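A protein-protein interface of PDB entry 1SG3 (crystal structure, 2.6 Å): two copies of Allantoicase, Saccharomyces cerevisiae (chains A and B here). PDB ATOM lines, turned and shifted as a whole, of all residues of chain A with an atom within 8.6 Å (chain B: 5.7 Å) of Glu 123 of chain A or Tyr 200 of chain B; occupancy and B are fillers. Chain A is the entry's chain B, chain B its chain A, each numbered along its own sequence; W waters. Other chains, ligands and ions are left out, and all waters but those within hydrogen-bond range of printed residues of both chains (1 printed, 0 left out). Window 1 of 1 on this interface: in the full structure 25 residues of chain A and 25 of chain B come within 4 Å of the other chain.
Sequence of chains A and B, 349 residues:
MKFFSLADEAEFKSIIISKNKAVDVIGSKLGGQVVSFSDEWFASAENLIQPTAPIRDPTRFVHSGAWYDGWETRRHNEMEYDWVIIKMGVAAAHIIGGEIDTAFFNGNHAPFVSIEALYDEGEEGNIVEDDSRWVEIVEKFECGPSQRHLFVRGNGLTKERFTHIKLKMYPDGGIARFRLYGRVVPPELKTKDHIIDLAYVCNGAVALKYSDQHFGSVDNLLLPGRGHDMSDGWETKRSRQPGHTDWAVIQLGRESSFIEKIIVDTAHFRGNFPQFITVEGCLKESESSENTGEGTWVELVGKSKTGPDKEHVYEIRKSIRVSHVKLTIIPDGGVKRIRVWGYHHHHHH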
ATOM      1  N   GLN A  33     -19.018 -24.164 -10.917  1.00  0.00           N
ATOM      2  CA  GLN A  33     -18.051 -23.290 -11.554  1.00  0.00           C
ATOM      3  C   GLN A  33     -18.336 -23.114 -13.040  1.00  0.00           C
ATOM      4  O   GLN A  33     -18.699 -24.069 -13.723  1.00  0.00           O
ATOM      5  CB  GLN A  33     -16.654 -23.861 -11.348  1.00  0.00           C
ATOM      6  CG  GLN A  33     -15.543 -22.870 -11.589  1.00  0.00           C
ATOM      7  CD  GLN A  33     -14.223 -23.323 -10.983  1.00  0.00           C
ATOM      8  OE1 GLN A  33     -13.156 -22.760 -11.279  1.00  0.00           O
ATOM      9  NE2 GLN A  33     -14.287 -24.342 -10.123  1.00  0.00           N
ATOM     10  N   VAL A  35     -17.490 -22.922 -16.739  1.00  0.00           N
ATOM     11  CA  VAL A  35     -16.404 -23.495 -17.522  1.00  0.00           C
ATOM     12  C   VAL A  35     -16.117 -22.595 -18.711  1.00  0.00           C
ATOM     13  O   VAL A  35     -14.967 -22.380 -19.076  1.00  0.00           O
ATOM     14  CB  VAL A  35     -16.761 -24.914 -18.008  1.00  0.00           C
ATOM     15  CG1 VAL A  35     -15.653 -25.445 -18.917  1.00  0.00           C
ATOM     16  CG2 VAL A  35     -16.988 -25.825 -16.814  1.00  0.00           C
ATOM     17  N   LYS A  87     -19.947 -26.501 -14.673  1.00  0.00           N
ATOM     18  CA  LYS A  87     -19.596 -27.808 -14.148  1.00  0.00           C
ATOM     19  C   LYS A  87     -20.168 -27.939 -12.746  1.00  0.00           C
ATOM     20  O   LYS A  87     -20.070 -27.013 -11.946  1.00  0.00           O
ATOM     21  CB  LYS A  87     -18.081 -27.961 -14.088  1.00  0.00           C
ATOM     22  CG  LYS A  87     -17.605 -29.293 -13.557  1.00  0.00           C
ATOM     23  CD  LYS A  87     -16.101 -29.371 -13.613  1.00  0.00           C
ATOM     24  CE  LYS A  87     -15.600 -30.742 -13.175  1.00  0.00           C
ATOM     25  NZ  LYS A  87     -16.034 -31.083 -11.789  1.00  0.00           N
ATOM     26  N   MET A  88     -20.775 -29.085 -12.461  1.00  0.00           N
ATOM     27  CA  MET A  88     -21.353 -29.362 -11.151  1.00  0.00           C
ATOM     28  C   MET A  88     -20.272 -29.413 -10.075  1.00  0.00           C
ATOM     29  O   MET A  88     -19.159 -29.879 -10.336  1.00  0.00           O
ATOM     30  CB  MET A  88     -22.061 -30.716 -11.164  1.00  0.00           C
ATOM     31  CG  MET A  88     -23.539 -30.695 -11.482  1.00  0.00           C
ATOM     32  SD  MET A  88     -24.164 -32.369 -11.474  1.00  0.00           S
ATOM     33  CE  MET A  88     -24.861 -32.451 -13.098  1.00  0.00           C
ATOM     34  N   ASP A 120     -19.184 -36.304 -18.194  1.00  0.00           N
ATOM     35  CA  ASP A 120     -17.780 -36.510 -18.505  1.00  0.00           C
ATOM     36  C   ASP A 120     -17.043 -37.077 -17.308  1.00  0.00           C
ATOM     37  O   ASP A 120     -17.030 -36.484 -16.227  1.00  0.00           O
ATOM     38  CB  ASP A 120     -17.100 -35.216 -18.951  1.00  0.00           C
ATOM     39  CG  ASP A 120     -15.686 -35.458 -19.465  1.00  0.00           C
ATOM     40  OD1 ASP A 120     -15.535 -36.176 -20.476  1.00  0.00           O
ATOM     41  OD2 ASP A 120     -14.725 -34.944 -18.858  1.00  0.00           O
ATOM     42  N   GLU A 121     -16.428 -38.232 -17.536  1.00  0.00           N
ATOM     43  CA  GLU A 121     -15.667 -38.974 -16.537  1.00  0.00           C
ATOM     44  C   GLU A 121     -14.715 -38.118 -15.699  1.00  0.00           C
ATOM     45  O   GLU A 121     -15.043 -37.732 -14.574  1.00  0.00           O
ATOM     46  CB  GLU A 121     -14.874 -40.080 -17.239  1.00  0.00           C
ATOM     47  CG  GLU A 121     -15.671 -40.824 -18.319  1.00  0.00           C
ATOM     48  CD  GLU A 121     -16.856 -41.611 -17.768  1.00  0.00           C
ATOM     49  OE1 GLU A 121     -17.623 -42.173 -18.577  1.00  0.00           O
ATOM     50  OE2 GLU A 121     -17.022 -41.673 -16.530  1.00  0.00           O
ATOM     51  N   GLY A 122     -13.533 -37.832 -16.242  1.00  0.00           N
ATOM     52  CA  GLY A 122     -12.564 -37.038 -15.506  1.00  0.00           C
ATOM     53  C   GLY A 122     -12.227 -35.693 -16.121  1.00  0.00           C
ATOM     54  O   GLY A 122     -12.418 -35.480 -17.320  1.00  0.00           O
ATOM     55  N   GLU A 123     -11.724 -34.785 -15.287  1.00  0.00           N
ATOM     56  CA  GLU A 123     -11.342 -33.441 -15.716  1.00  0.00           C
ATOM     57  C   GLU A 123     -10.271 -33.487 -16.815  1.00  0.00           C
ATOM     58  O   GLU A 123      -9.110 -33.121 -16.597  1.00  0.00           O
ATOM     59  CB  GLU A 123     -10.835 -32.645 -14.509  1.00  0.00           C
ATOM     60  CG  GLU A 123     -10.406 -31.204 -14.811  1.00  0.00           C
ATOM     61  CD  GLU A 123     -11.546 -30.307 -15.309  1.00  0.00           C
ATOM     62  OE1 GLU A 123     -12.593 -30.223 -14.627  1.00  0.00           O
ATOM     63  OE2 GLU A 123     -11.386 -29.671 -16.377  1.00  0.00           O
ATOM     64  N   GLU A 124     -10.682 -33.945 -17.996  1.00  0.00           N
ATOM     65  CA  GLU A 124      -9.802 -34.062 -19.157  1.00  0.00           C
ATOM     66  C   GLU A 124      -9.436 -32.680 -19.657  1.00  0.00           C
ATOM     67  O   GLU A 124      -8.363 -32.466 -20.211  1.00  0.00           O
ATOM     68  CB  GLU A 124     -10.513 -34.839 -20.270  1.00  0.00           C
ATOM     69  CG  GLU A 124     -11.907 -34.315 -20.586  1.00  0.00           C
ATOM     70  CD  GLU A 124     -12.686 -35.241 -21.508  1.00  0.00           C
ATOM     71  OE1 GLU A 124     -12.783 -36.450 -21.193  1.00  0.00           O
ATOM     72  OE2 GLU A 124     -13.212 -34.758 -22.538  1.00  0.00           O
ATOM     73  N   GLY A 125     -10.358 -31.750 -19.451  1.00  0.00           N
ATOM     74  CA  GLY A 125     -10.164 -30.379 -19.868  1.00  0.00           C
ATOM     75  C   GLY A 125     -11.495 -29.693 -19.693  1.00  0.00           C
ATOM     76  O   GLY A 125     -12.399 -30.256 -19.084  1.00  0.00           O
ATOM     77  N   ASN A 126     -11.627 -28.480 -20.206  1.00  0.00           N
ATOM     78  CA  ASN A 126     -12.890 -27.781 -20.094  1.00  0.00           C
ATOM     79  C   ASN A 126     -13.771 -28.208 -21.269  1.00  0.00           C
ATOM     80  O   ASN A 126     -13.367 -28.099 -22.425  1.00  0.00           O
ATOM     81  CB  ASN A 126     -12.665 -26.270 -20.094  1.00  0.00           C
ATOM     82  CG  ASN A 126     -11.929 -25.785 -18.843  1.00  0.00           C
ATOM     83  OD1 ASN A 126     -12.236 -26.194 -17.711  1.00  0.00           O
ATOM     84  ND2 ASN A 126     -10.967 -24.896 -19.042  1.00  0.00           N
ATOM     85  N   ILE A 127     -14.960 -28.719 -20.961  1.00  0.00           N
ATOM     86  CA  ILE A 127     -15.883 -29.188 -21.983  1.00  0.00           C
ATOM     87  C   ILE A 127     -16.191 -28.080 -22.980  1.00  0.00           C
ATOM     88  O   ILE A 127     -16.150 -26.907 -22.629  1.00  0.00           O
ATOM     89  CB  ILE A 127     -17.211 -29.681 -21.344  1.00  0.00           C
ATOM     90  CG1 ILE A 127     -16.935 -30.835 -20.377  1.00  0.00           C
ATOM     91  CG2 ILE A 127     -18.175 -30.144 -22.424  1.00  0.00           C
ATOM     92  CD1 ILE A 127     -16.340 -32.069 -21.028  1.00  0.00           C
ATOM     93  N   THR A 163     -22.572 -34.443 -15.189  1.00  0.00           N
ATOM     94  CA  THR A 163     -21.534 -33.730 -14.457  1.00  0.00           C
ATOM     95  C   THR A 163     -21.429 -32.257 -14.850  1.00  0.00           C
ATOM     96  O   THR A 163     -20.916 -31.438 -14.094  1.00  0.00           O
ATOM     97  CB  THR A 163     -20.170 -34.375 -14.695  1.00  0.00           C
ATOM     98  OG1 THR A 163     -19.892 -34.384 -16.101  1.00  0.00           O
ATOM     99  CG2 THR A 163     -20.156 -35.794 -14.166  1.00  0.00           C
ATOM    100  N   HIS A 164     -21.896 -31.926 -16.046  1.00  0.00           N
ATOM    101  CA  HIS A 164     -21.859 -30.552 -16.536  1.00  0.00           C
ATOM    102  C   HIS A 164     -23.210 -30.196 -17.132  1.00  0.00           C
ATOM    103  O   HIS A 164     -23.912 -31.068 -17.649  1.00  0.00           O
ATOM    104  CB  HIS A 164     -20.831 -30.383 -17.660  1.00  0.00           C
ATOM    105  CG  HIS A 164     -19.439 -30.781 -17.295  1.00  0.00           C
ATOM    106  ND1 HIS A 164     -18.359 -29.946 -17.485  1.00  0.00           N
ATOM    107  CD2 HIS A 164     -18.937 -31.947 -16.829  1.00  0.00           C
ATOM    108  CE1 HIS A 164     -17.251 -30.581 -17.153  1.00  0.00           C
ATOM    109  NE2 HIS A 164     -17.573 -31.798 -16.754  1.00  0.00           N
ATOM    110  N   PRO B 187      -5.413 -37.646 -13.551  1.00  0.00           N
ATOM    111  CA  PRO B 187      -6.528 -38.535 -13.206  1.00  0.00           C
ATOM    112  C   PRO B 187      -6.437 -39.898 -13.891  1.00  0.00           C
ATOM    113  O   PRO B 187      -7.030 -40.869 -13.426  1.00  0.00           O
ATOM    114  CB  PRO B 187      -7.742 -37.743 -13.669  1.00  0.00           C
ATOM    115  CG  PRO B 187      -7.218 -37.066 -14.906  1.00  0.00           C
ATOM    116  CD  PRO B 187      -5.875 -36.553 -14.427  1.00  0.00           C
ATOM    117  N   ASP B 197      -7.202 -32.532 -22.738  1.00  0.00           N
ATOM    118  CA  ASP B 197      -6.434 -31.310 -22.929  1.00  0.00           C
ATOM    119  C   ASP B 197      -5.011 -31.601 -22.459  1.00  0.00           C
ATOM    120  O   ASP B 197      -4.736 -31.622 -21.261  1.00  0.00           O
ATOM    121  CB  ASP B 197      -7.024 -30.159 -22.110  1.00  0.00           C
ATOM    122  CG  ASP B 197      -6.429 -28.815 -22.493  1.00  0.00           C
ATOM    123  OD1 ASP B 197      -5.363 -28.817 -23.148  1.00  0.00           O
ATOM    124  OD2 ASP B 197      -7.015 -27.764 -22.142  1.00  0.00           O
ATOM    125  N   LEU B 198      -4.112 -31.831 -23.406  1.00  0.00           N
ATOM    126  CA  LEU B 198      -2.735 -32.149 -23.087  1.00  0.00           C
ATOM    127  C   LEU B 198      -1.975 -31.009 -22.414  1.00  0.00           C
ATOM    128  O   LEU B 198      -0.946 -31.236 -21.766  1.00  0.00           O
ATOM    129  CB  LEU B 198      -2.002 -32.577 -24.366  1.00  0.00           C
ATOM    130  CG  LEU B 198      -2.525 -33.821 -25.106  1.00  0.00           C
ATOM    131  CD1 LEU B 198      -1.886 -33.912 -26.466  1.00  0.00           C
ATOM    132  CD2 LEU B 198      -2.226 -35.076 -24.301  1.00  0.00           C
ATOM    133  N   ALA B 199      -2.478 -29.785 -22.556  1.00  0.00           N
ATOM    134  CA  ALA B 199      -1.801 -28.622 -21.970  1.00  0.00           C
ATOM    135  C   ALA B 199      -2.524 -28.104 -20.736  1.00  0.00           C
ATOM    136  O   ALA B 199      -2.284 -26.990 -20.261  1.00  0.00           O
ATOM    137  CB  ALA B 199      -1.682 -27.518 -23.012  1.00  0.00           C
ATOM    138  N   TYR B 200      -3.409 -28.943 -20.220  1.00  0.00           N
ATOM    139  CA  TYR B 200      -4.206 -28.627 -19.058  1.00  0.00           C
ATOM    140  C   TYR B 200      -3.389 -28.942 -17.809  1.00  0.00           C
ATOM    141  O   TYR B 200      -2.816 -30.031 -17.690  1.00  0.00           O
ATOM    142  CB  TYR B 200      -5.492 -29.454 -19.114  1.00  0.00           C
ATOM    143  CG  TYR B 200      -6.599 -28.956 -18.224  1.00  0.00           C
ATOM    144  CD1 TYR B 200      -6.919 -27.596 -18.165  1.00  0.00           C
ATOM    145  CD2 TYR B 200      -7.340 -29.841 -17.444  1.00  0.00           C
ATOM    146  CE1 TYR B 200      -7.950 -27.136 -17.348  1.00  0.00           C
ATOM    147  CE2 TYR B 200      -8.366 -29.389 -16.627  1.00  0.00           C
ATOM    148  CZ  TYR B 200      -8.663 -28.041 -16.583  1.00  0.00           C
ATOM    149  OH  TYR B 200      -9.665 -27.604 -15.759  1.00  0.00           O
ATOM    150  N   VAL B 201      -3.331 -27.972 -16.892  1.00  0.00           N
ATOM    151  CA  VAL B 201      -2.581 -28.104 -15.642  1.00  0.00           C
ATOM    152  C   VAL B 201      -3.076 -29.285 -14.803  1.00  0.00           C
ATOM    153  O   VAL B 201      -2.283 -29.973 -14.156  1.00  0.00           O
ATOM    154  CB  VAL B 201      -2.659 -26.795 -14.786  1.00  0.00           C
ATOM    155  CG1 VAL B 201      -4.091 -26.545 -14.302  1.00  0.00           C
ATOM    156  CG2 VAL B 201      -1.707 -26.886 -13.604  1.00  0.00           C
ATOM    157  N   CYS B 202      -4.384 -29.513 -14.820  1.00  0.00           N
ATOM    158  CA  CYS B 202      -4.974 -30.609 -14.068  1.00  0.00           C
ATOM    159  C   CYS B 202      -4.564 -31.956 -14.671  1.00  0.00           C
ATOM    160  O   CYS B 202      -4.845 -33.007 -14.107  1.00  0.00           O
ATOM    161  CB  CYS B 202      -6.502 -30.468 -14.041  1.00  0.00           C
ATOM    162  SG  CYS B 202      -7.108 -29.035 -13.085  1.00  0.00           S
ATOM    163  N   ASN B 203      -3.896 -31.917 -15.821  1.00  0.00           N
ATOM    164  CA  ASN B 203      -3.426 -33.135 -16.464  1.00  0.00           C
ATOM    165  C   ASN B 203      -1.913 -33.285 -16.347  1.00  0.00           C
ATOM    166  O   ASN B 203      -1.344 -34.257 -16.855  1.00  0.00           O
ATOM    167  CB  ASN B 203      -3.831 -33.174 -17.936  1.00  0.00           C
ATOM    168  CG  ASN B 203      -5.283 -33.560 -18.124  1.00  0.00           C
ATOM    169  OD1 ASN B 203      -5.776 -34.480 -17.466  1.00  0.00           O
ATOM    170  ND2 ASN B 203      -5.976 -32.867 -19.025  1.00  0.00           N
ATOM    171  N   GLY B 204      -1.262 -32.327 -15.682  1.00  0.00           N
ATOM    172  CA  GLY B 204       0.178 -32.398 -15.506  1.00  0.00           C
ATOM    173  C   GLY B 204       1.026 -31.459 -16.347  1.00  0.00           C
ATOM    174  O   GLY B 204       2.254 -31.527 -16.299  1.00  0.00           O
ATOM    175  N   ALA B 205       0.393 -30.585 -17.121  1.00  0.00           N
ATOM    176  CA  ALA B 205       1.152 -29.640 -17.934  1.00  0.00           C
ATOM    177  C   ALA B 205       1.631 -28.497 -17.058  1.00  0.00           C
ATOM    178  O   ALA B 205       1.021 -28.175 -16.046  1.00  0.00           O
ATOM    179  CB  ALA B 205       0.294 -29.102 -19.058  1.00  0.00           C
ATOM    180  N   LEU B 222      -2.821 -22.494 -18.730  1.00  0.00           N
ATOM    181  CA  LEU B 222      -3.236 -23.873 -18.529  1.00  0.00           C
ATOM    182  C   LEU B 222      -4.301 -24.087 -17.468  1.00  0.00           C
ATOM    183  O   LEU B 222      -4.487 -25.214 -17.004  1.00  0.00           O
ATOM    184  CB  LEU B 222      -2.015 -24.706 -18.179  1.00  0.00           C
ATOM    185  CG  LEU B 222      -0.756 -24.297 -18.943  1.00  0.00           C
ATOM    186  CD1 LEU B 222       0.372 -25.245 -18.603  1.00  0.00           C
ATOM    187  CD2 LEU B 222      -1.033 -24.322 -20.432  1.00  0.00           C
ATOM    188  N   LEU B 223      -5.024 -23.030 -17.108  1.00  0.00           N
ATOM    189  CA  LEU B 223      -6.037 -23.131 -16.064  1.00  0.00           C
ATOM    190  C   LEU B 223      -7.469 -23.451 -16.506  1.00  0.00           C
ATOM    191  O   LEU B 223      -7.800 -23.392 -17.694  1.00  0.00           O
ATOM    192  CB  LEU B 223      -6.054 -21.834 -15.257  1.00  0.00           C
ATOM    193  CG  LEU B 223      -4.761 -21.442 -14.556  1.00  0.00           C
ATOM    194  CD1 LEU B 223      -4.869 -20.005 -14.113  1.00  0.00           C
ATOM    195  CD2 LEU B 223      -4.507 -22.354 -13.369  1.00  0.00           C
ATOM    196  N   PRO B 224      -8.336 -23.806 -15.533  1.00  0.00           N
ATOM    197  CA  PRO B 224      -9.743 -24.128 -15.779  1.00  0.00           C
ATOM    198  C   PRO B 224     -10.549 -22.844 -15.978  1.00  0.00           C
ATOM    199  O   PRO B 224     -10.169 -21.785 -15.472  1.00  0.00           O
ATOM    200  CB  PRO B 224     -10.154 -24.887 -14.515  1.00  0.00           C
ATOM    201  CG  PRO B 224      -9.269 -24.325 -13.477  1.00  0.00           C
ATOM    202  CD  PRO B 224      -7.946 -24.225 -14.173  1.00  0.00           C
ATOM    203  N   GLY B 225     -11.649 -22.945 -16.723  1.00  0.00           N
ATOM    204  CA  GLY B 225     -12.484 -21.785 -16.991  1.00  0.00           C
ATOM    205  C   GLY B 225     -11.860 -20.770 -17.942  1.00  0.00           C
ATOM    206  O   GLY B 225     -10.706 -20.917 -18.357  1.00  0.00           O
ATOM    207  N   GLY B 253       1.384 -32.322 -20.130  1.00  0.00           N
ATOM    208  CA  GLY B 253       1.506 -33.279 -19.049  1.00  0.00           C
ATOM    209  C   GLY B 253       1.596 -34.715 -19.537  1.00  0.00           C
ATOM    210  O   GLY B 253       1.611 -35.644 -18.736  1.00  0.00           O
ATOM    211  N   ARG B 339      -5.409 -24.343 -25.337  1.00  0.00           N
ATOM    212  CA  ARG B 339      -5.853 -25.725 -25.128  1.00  0.00           C
ATOM    213  C   ARG B 339      -5.290 -26.572 -26.256  1.00  0.00           C
ATOM    214  O   ARG B 339      -5.147 -26.095 -27.381  1.00  0.00           O
ATOM    215  CB  ARG B 339      -7.378 -25.852 -25.177  1.00  0.00           C
ATOM    216  CG  ARG B 339      -8.160 -24.845 -24.368  1.00  0.00           C
ATOM    217  CD  ARG B 339      -7.765 -24.863 -22.912  1.00  0.00           C
ATOM    218  NE  ARG B 339      -8.662 -24.057 -22.084  1.00  0.00           N
ATOM    219  CZ  ARG B 339      -8.426 -23.786 -20.803  1.00  0.00           C
ATOM    220  NH1 ARG B 339      -7.331 -24.254 -20.223  1.00  0.00           N
ATOM    221  NH2 ARG B 339      -9.277 -23.050 -20.097  1.00  0.00           N
HETATM  222  O   HOH W   1      -9.675 -27.588 -21.632  1.00  0.00           O
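Of chain B, only Tyr 200 and Asn 203 come within 4 Å of Glu 123 of chain A.
Of the printed residues of chain A, Tyr 200 of chain B touches Glu 123 (2.8 Å), Glu 124 (3.9 Å), Gly 125 (3.8 Å) and Asn 126 (3.5 Å).
No residue of chain A comes within 4 Å of Ala 199 of chain B.
Of the printed residues of chain A, Pro 224 of chain B touches Asn 126 (3.6 Å).
Of the printed residues of chain A, Gly 225 of chain B touches Val 35 and Asn 126.
Printed residues of chain B within 4 Å of Val 35 of chain A: Gly 225.
Printed residues of chain A within 4 Å of Arg 339 of chain B: Asn 126.
Printed residues of chain B within 4 Å of Gly 125 of chain A: Asp 197 (3.9 Å) and Tyr 200 (3.8 Å).
Thr 163 of chain A touches none of the printed residues of chain B.
The nearest residue of chain A that does not touch Tyr 200 of chain B is Lys 87 of chain A (7.0 Å).
No position is printed for both chains.
Of the 13 pairs that touch across the chains among the printed residues, none has its exchanged pair printed and touching as well.
Among the printed residues, merely in contact across the chains: Val 35 of chain A with Gly 225 of chain B, Asn 126 of chain A with Tyr 200 of chain B, Asn 126 of chain A with Pro 224 of chain B, Glu 123 of chain A with Asn 203 of chain B, Asn 126 of chain A with Leu 223 of chain B, Gly 125 of chain A with Tyr 200 of chain B, Gly 125 of chain A with Asp 197 of chain B and Glu 124 of chain A with Tyr 200 of chain B.
The side-chain carboxylate (OD1) of Asp 197 of chain B is in hydrogen-bond range of the backbone NH (N) of Ala 199 of chain B (3.1 Å).
ND2 of Asn 203 of chain B sits at hydrogen-bond distance from O of Asp 197 of chain B, 2.8 Å away.
The backbone carbonyl oxygen (O) of Gly 225 of chain B is in hydrogen-bond range of the guanidinium group (NH2) of Arg 339 of chain B (3.1 Å).
The backbone carbonyl oxygen of Tyr 200 of chain B sits at hydrogen-bond distance from the backbone NH of Ala 205 of chain B.
NH1 of Arg 339 of chain B is in hydrogen-bond range of O of Leu 223 of chain B.
NH2 of Arg 339 of chain B sits close to ND2 of Asn 126 of chain A (2.7 Å).
The backbone carbonyl oxygen (O) of Glu 124 of chain A is in hydrogen-bond range of the side-chain amide nitrogen (ND2) of Asn 203 of chain B (2.7 Å).
N of Asp 197 of chain B is in hydrogen-bond range of O of Glu 124 of chain A, at 2.8 Å.
OE2 of Glu 123 of chain A sits at hydrogen-bond distance from OH of Tyr 200 of chain B (2.8 Å).
ND2 of Asn 126 of chain A sits close to N of Gly 225 of chain B (3.1 Å).
Hydrophobic or aromatic side chains of chain B within 4 Å of the printed part of chain A: Tyr 200.
Of the 14 printed residues of chain A, 5 touch a printed residue of chain B.
Among the printed residues, 13 pairs touch across the chains.
Among the printed residues, no Asp or Glu carboxylate lies within 4 Å of a Lys or Arg side-chain nitrogen of the other chain.
Water W1 bridges the backbone NH of Asn 126 of chain A and the side-chain carboxylate of Asp 197 of chain B.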
